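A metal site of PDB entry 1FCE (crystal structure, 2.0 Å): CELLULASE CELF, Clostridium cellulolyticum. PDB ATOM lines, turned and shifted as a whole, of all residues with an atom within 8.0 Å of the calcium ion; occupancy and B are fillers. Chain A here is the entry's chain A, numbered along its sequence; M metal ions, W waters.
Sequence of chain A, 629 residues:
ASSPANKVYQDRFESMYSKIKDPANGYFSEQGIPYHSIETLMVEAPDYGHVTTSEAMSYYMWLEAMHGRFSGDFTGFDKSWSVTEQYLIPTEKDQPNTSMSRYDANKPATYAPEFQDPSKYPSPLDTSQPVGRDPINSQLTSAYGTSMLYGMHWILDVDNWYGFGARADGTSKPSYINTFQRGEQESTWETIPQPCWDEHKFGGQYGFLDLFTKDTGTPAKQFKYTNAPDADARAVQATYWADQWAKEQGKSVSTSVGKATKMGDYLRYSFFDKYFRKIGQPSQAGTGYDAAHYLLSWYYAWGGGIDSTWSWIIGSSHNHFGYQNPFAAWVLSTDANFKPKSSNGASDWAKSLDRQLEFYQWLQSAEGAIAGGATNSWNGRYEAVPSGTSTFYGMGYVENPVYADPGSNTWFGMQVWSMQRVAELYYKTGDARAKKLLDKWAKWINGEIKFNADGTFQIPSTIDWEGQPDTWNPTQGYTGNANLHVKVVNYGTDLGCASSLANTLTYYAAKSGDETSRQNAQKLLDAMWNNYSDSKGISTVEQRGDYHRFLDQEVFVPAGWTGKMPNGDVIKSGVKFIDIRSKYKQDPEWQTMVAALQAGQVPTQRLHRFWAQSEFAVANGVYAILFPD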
ATOM      1  N   GLN A 116       4.871 -12.091 -26.104  1.00  0.00           N
ATOM      2  CA  GLN A 116       3.861 -12.268 -27.140  1.00  0.00           C
ATOM      3  C   GLN A 116       2.814 -13.330 -26.817  1.00  0.00           C
ATOM      4  O   GLN A 116       2.024 -13.701 -27.664  1.00  0.00           O
ATOM      5  CB  GLN A 116       4.524 -12.563 -28.483  1.00  0.00           C
ATOM      6  CG  GLN A 116       5.175 -11.346 -29.137  1.00  0.00           C
ATOM      7  CD  GLN A 116       6.302 -10.768 -28.310  1.00  0.00           C
ATOM      8  OE1 GLN A 116       7.317 -11.429 -28.097  1.00  0.00           O
ATOM      9  NE2 GLN A 116       6.120  -9.546 -27.816  1.00  0.00           N
ATOM     10  N   ASP A 117       2.829 -13.832 -25.590  1.00  0.00           N
ATOM     11  CA  ASP A 117       1.831 -14.799 -25.172  1.00  0.00           C
ATOM     12  C   ASP A 117       1.606 -14.627 -23.681  1.00  0.00           C
ATOM     13  O   ASP A 117       2.556 -14.579 -22.910  1.00  0.00           O
ATOM     14  CB  ASP A 117       2.255 -16.238 -25.476  1.00  0.00           C
ATOM     15  CG  ASP A 117       1.087 -17.193 -25.418  1.00  0.00           C
ATOM     16  OD1 ASP A 117       0.315 -17.231 -26.411  1.00  0.00           O
ATOM     17  OD2 ASP A 117       0.885 -17.864 -24.389  1.00  0.00           O
ATOM     18  N   PRO A 118       0.336 -14.540 -23.272  1.00  0.00           N
ATOM     19  CA  PRO A 118      -0.012 -14.380 -21.857  1.00  0.00           C
ATOM     20  C   PRO A 118       0.556 -15.463 -20.935  1.00  0.00           C
ATOM     21  O   PRO A 118       0.725 -15.224 -19.740  1.00  0.00           O
ATOM     22  CB  PRO A 118      -1.549 -14.408 -21.874  1.00  0.00           C
ATOM     23  CG  PRO A 118      -1.885 -13.878 -23.230  1.00  0.00           C
ATOM     24  CD  PRO A 118      -0.875 -14.567 -24.110  1.00  0.00           C
ATOM     25  N   GLY A 183       0.464  -8.245 -22.582  1.00  0.00           N
ATOM     26  CA  GLY A 183       0.876  -8.214 -23.979  1.00  0.00           C
ATOM     27  C   GLY A 183      -0.121  -8.227 -25.114  1.00  0.00           C
ATOM     28  O   GLY A 183      -1.346  -8.290 -24.912  1.00  0.00           O
ATOM     29  N   GLU A 184       0.442  -8.292 -26.321  1.00  0.00           N
ATOM     30  CA  GLU A 184      -0.311  -8.252 -27.566  1.00  0.00           C
ATOM     31  C   GLU A 184      -1.362  -9.330 -27.801  1.00  0.00           C
ATOM     32  O   GLU A 184      -2.329  -9.112 -28.538  1.00  0.00           O
ATOM     33  CB  GLU A 184       0.648  -8.220 -28.768  1.00  0.00           C
ATOM     34  CG  GLU A 184       1.416  -9.497 -28.974  1.00  0.00           C
ATOM     35  CD  GLU A 184       2.224  -9.505 -30.261  1.00  0.00           C
ATOM     36  OE1 GLU A 184       2.782  -8.450 -30.625  1.00  0.00           O
ATOM     37  OE2 GLU A 184       2.292 -10.581 -30.900  1.00  0.00           O
ATOM     38  N   GLN A 185      -1.169 -10.505 -27.229  1.00  0.00           N
ATOM     39  CA  GLN A 185      -2.133 -11.567 -27.424  1.00  0.00           C
ATOM     40  C   GLN A 185      -3.188 -11.642 -26.329  1.00  0.00           C
ATOM     41  O   GLN A 185      -4.003 -12.546 -26.310  1.00  0.00           O
ATOM     42  CB  GLN A 185      -1.443 -12.921 -27.646  1.00  0.00           C
ATOM     43  CG  GLN A 185      -1.135 -13.180 -29.123  1.00  0.00           C
ATOM     44  CD  GLN A 185      -2.403 -13.406 -29.979  1.00  0.00           C
ATOM     45  OE1 GLN A 185      -3.469 -13.773 -29.460  1.00  0.00           O
ATOM     46  NE2 GLN A 185      -2.288 -13.185 -31.272  1.00  0.00           N
ATOM     47  N   GLU A 186      -3.176 -10.699 -25.395  1.00  0.00           N
ATOM     48  CA  GLU A 186      -4.204 -10.737 -24.362  1.00  0.00           C
ATOM     49  C   GLU A 186      -5.404  -9.905 -24.802  1.00  0.00           C
ATOM     50  O   GLU A 186      -5.382  -8.682 -24.711  1.00  0.00           O
ATOM     51  CB  GLU A 186      -3.677 -10.236 -23.022  1.00  0.00           C
ATOM     52  CG  GLU A 186      -4.609 -10.539 -21.864  1.00  0.00           C
ATOM     53  CD  GLU A 186      -4.184  -9.860 -20.581  1.00  0.00           C
ATOM     54  OE1 GLU A 186      -3.765  -8.689 -20.658  1.00  0.00           O
ATOM     55  OE2 GLU A 186      -4.272 -10.486 -19.503  1.00  0.00           O
ATOM     56  N   SER A 187      -6.421 -10.570 -25.343  1.00  0.00           N
ATOM     57  CA  SER A 187      -7.633  -9.875 -25.773  1.00  0.00           C
ATOM     58  C   SER A 187      -8.456  -9.532 -24.535  1.00  0.00           C
ATOM     59  O   SER A 187      -8.082  -9.882 -23.404  1.00  0.00           O
ATOM     60  CB  SER A 187      -8.446 -10.794 -26.690  1.00  0.00           C
ATOM     61  OG  SER A 187      -8.999 -11.869 -25.968  1.00  0.00           O
ATOM     62  N   THR A 188      -9.595  -8.867 -24.740  1.00  0.00           N
ATOM     63  CA  THR A 188     -10.492  -8.491 -23.645  1.00  0.00           C
ATOM     64  C   THR A 188     -11.027  -9.747 -22.955  1.00  0.00           C
ATOM     65  O   THR A 188     -11.476  -9.672 -21.817  1.00  0.00           O
ATOM     66  CB  THR A 188     -11.739  -7.793 -24.154  1.00  0.00           C
ATOM     67  OG1 THR A 188     -11.414  -7.050 -25.335  1.00  0.00           O
ATOM     68  CG2 THR A 188     -12.257  -6.849 -23.114  1.00  0.00           C
ATOM     69  N   TRP A 189     -11.015 -10.868 -23.683  1.00  0.00           N
ATOM     70  CA  TRP A 189     -11.516 -12.141 -23.183  1.00  0.00           C
ATOM     71  C   TRP A 189     -10.504 -12.916 -22.340  1.00  0.00           C
ATOM     72  O   TRP A 189     -10.867 -13.875 -21.668  1.00  0.00           O
ATOM     73  CB  TRP A 189     -11.912 -13.026 -24.366  1.00  0.00           C
ATOM     74  CG  TRP A 189     -12.863 -12.366 -25.307  1.00  0.00           C
ATOM     75  CD1 TRP A 189     -12.550 -11.718 -26.473  1.00  0.00           C
ATOM     76  CD2 TRP A 189     -14.291 -12.294 -25.166  1.00  0.00           C
ATOM     77  NE1 TRP A 189     -13.706 -11.257 -27.068  1.00  0.00           N
ATOM     78  CE2 TRP A 189     -14.778 -11.590 -26.280  1.00  0.00           C
ATOM     79  CE3 TRP A 189     -15.191 -12.757 -24.198  1.00  0.00           C
ATOM     80  CZ2 TRP A 189     -16.144 -11.345 -26.462  1.00  0.00           C
ATOM     81  CZ3 TRP A 189     -16.556 -12.511 -24.380  1.00  0.00           C
ATOM     82  CH2 TRP A 189     -17.010 -11.804 -25.518  1.00  0.00           C
ATOM     83  N   GLU A 190      -9.243 -12.471 -22.359  1.00  0.00           N
ATOM     84  CA  GLU A 190      -8.175 -13.183 -21.660  1.00  0.00           C
ATOM     85  C   GLU A 190      -7.543 -12.528 -20.444  1.00  0.00           C
ATOM     86  O   GLU A 190      -6.517 -13.008 -19.926  1.00  0.00           O
ATOM     87  CB  GLU A 190      -7.108 -13.529 -22.698  1.00  0.00           C
ATOM     88  CG  GLU A 190      -7.606 -14.467 -23.764  1.00  0.00           C
ATOM     89  CD  GLU A 190      -6.731 -14.448 -24.983  1.00  0.00           C
ATOM     90  OE1 GLU A 190      -6.996 -13.598 -25.850  1.00  0.00           O
ATOM     91  OE2 GLU A 190      -5.784 -15.261 -25.071  1.00  0.00           O
ATOM     92  N   ALA A 404      -2.836  -7.684 -31.148  1.00  0.00           N
ATOM     93  CA  ALA A 404      -2.927  -8.576 -32.305  1.00  0.00           C
ATOM     94  C   ALA A 404      -4.180  -9.433 -32.249  1.00  0.00           C
ATOM     95  O   ALA A 404      -4.461 -10.163 -33.194  1.00  0.00           O
ATOM     96  CB  ALA A 404      -1.693  -9.469 -32.360  1.00  0.00           C
ATOM     97  N   ASP A 405      -4.930  -9.333 -31.155  1.00  0.00           N
ATOM     98  CA  ASP A 405      -6.148 -10.135 -30.972  1.00  0.00           C
ATOM     99  C   ASP A 405      -7.398  -9.312 -30.570  1.00  0.00           C
ATOM    100  O   ASP A 405      -7.741  -9.242 -29.382  1.00  0.00           O
ATOM    101  CB  ASP A 405      -5.857 -11.218 -29.917  1.00  0.00           C
ATOM    102  CG  ASP A 405      -6.977 -12.262 -29.779  1.00  0.00           C
ATOM    103  OD1 ASP A 405      -7.974 -12.228 -30.528  1.00  0.00           O
ATOM    104  OD2 ASP A 405      -6.853 -13.139 -28.891  1.00  0.00           O
ATOM    105  N   PRO A 406      -8.050  -8.638 -31.534  1.00  0.00           N
ATOM    106  CA  PRO A 406      -7.753  -8.553 -32.966  1.00  0.00           C
ATOM    107  C   PRO A 406      -6.743  -7.425 -33.204  1.00  0.00           C
ATOM    108  O   PRO A 406      -6.475  -6.624 -32.304  1.00  0.00           O
ATOM    109  CB  PRO A 406      -9.118  -8.229 -33.569  1.00  0.00           C
ATOM    110  CG  PRO A 406      -9.693  -7.315 -32.575  1.00  0.00           C
ATOM    111  CD  PRO A 406      -9.346  -7.992 -31.248  1.00  0.00           C
ATOM    112  N   ARG A 549     -16.620 -16.691 -27.179  1.00  0.00           N
ATOM    113  CA  ARG A 549     -15.506 -16.670 -26.247  1.00  0.00           C
ATOM    114  C   ARG A 549     -15.936 -16.504 -24.775  1.00  0.00           C
ATOM    115  O   ARG A 549     -15.145 -16.720 -23.865  1.00  0.00           O
ATOM    116  CB  ARG A 549     -14.498 -15.595 -26.668  1.00  0.00           C
ATOM    117  CG  ARG A 549     -14.006 -15.825 -28.086  1.00  0.00           C
ATOM    118  CD  ARG A 549     -13.059 -14.741 -28.528  1.00  0.00           C
ATOM    119  NE  ARG A 549     -11.736 -14.909 -27.921  1.00  0.00           N
ATOM    120  CZ  ARG A 549     -10.644 -14.257 -28.323  1.00  0.00           C
ATOM    121  NH1 ARG A 549     -10.704 -13.379 -29.322  1.00  0.00           N
ATOM    122  NH2 ARG A 549      -9.473 -14.535 -27.761  1.00  0.00           N
ATOM    123  N   GLN A 553     -13.357 -19.381 -24.091  1.00  0.00           N
ATOM    124  CA  GLN A 553     -12.031 -18.780 -23.943  1.00  0.00           C
ATOM    125  C   GLN A 553     -11.401 -19.078 -22.602  1.00  0.00           C
ATOM    126  O   GLN A 553     -11.907 -18.670 -21.552  1.00  0.00           O
ATOM    127  CB  GLN A 553     -12.076 -17.259 -24.162  1.00  0.00           C
ATOM    128  CG  GLN A 553     -10.703 -16.585 -24.025  1.00  0.00           C
ATOM    129  CD  GLN A 553      -9.773 -16.998 -25.108  1.00  0.00           C
ATOM    130  OE1 GLN A 553     -10.005 -16.720 -26.274  1.00  0.00           O
ATOM    131  NE2 GLN A 553      -8.702 -17.694 -24.736  1.00  0.00           N
ATOM    132  N   GLU A 554     -10.326 -19.846 -22.639  1.00  0.00           N
ATOM    133  CA  GLU A 554      -9.593 -20.188 -21.428  1.00  0.00           C
ATOM    134  C   GLU A 554      -8.754 -18.987 -21.012  1.00  0.00           C
ATOM    135  O   GLU A 554      -8.225 -18.280 -21.862  1.00  0.00           O
ATOM    136  CB  GLU A 554      -8.684 -21.385 -21.690  1.00  0.00           C
ATOM    137  CG  GLU A 554      -8.030 -21.915 -20.417  1.00  0.00           C
ATOM    138  CD  GLU A 554      -7.091 -23.096 -20.681  1.00  0.00           C
ATOM    139  OE1 GLU A 554      -7.474 -23.992 -21.473  1.00  0.00           O
ATOM    140  OE2 GLU A 554      -5.978 -23.107 -20.093  1.00  0.00           O
HETATM  141 CA    CA M   1      -5.176 -14.311 -27.484  1.00  0.00          CA
HETATM  142  O   HOH W   1      -3.304 -15.870 -26.998  1.00  0.00           O
HETATM  143  O   HOH W   2      -6.481 -16.192 -28.350  1.00  0.00           O
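NH1 of Arg 549 lies within salt-bridge range of OD1 of Asp 405 (3.2 Å). The side-chain carboxylate of Glu 190 sits close to the guanidinium group of Arg 549, at 3.3 Å. OG of Ser 187 lies close to OE1 of Glu 190 (2.6 Å).
Three residues have an atom within 4 Å of the calcium ion: Gln 185, Glu 190 and Asp 405. Along chain A the residues within 4 Å of the calcium ion span positions 185 to 405. The nearest printed residue that does not touch the calcium ion is Arg 549 (4.3 Å).
The calcium ion is bound by the backbone carbonyl oxygen (O) of Gln 185 (2.4 Å). Water W2 is bound to the calcium ion (2.4 Å). OD2 of Asp 405 is bound to the calcium ion (2.5 Å). Water W1 binds the calcium ion. The calcium ion is bound by the side-chain carboxylate (OE1) of Glu 190 (2.5 Å). The calcium ion is bound by OE2 of Glu 190 (2.7 Å). The calcium ion is bound by the side-chain amide oxygen (OE1) of Gln 185 (2.7 Å). The calcium ion has seven donor atoms within binding distance.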
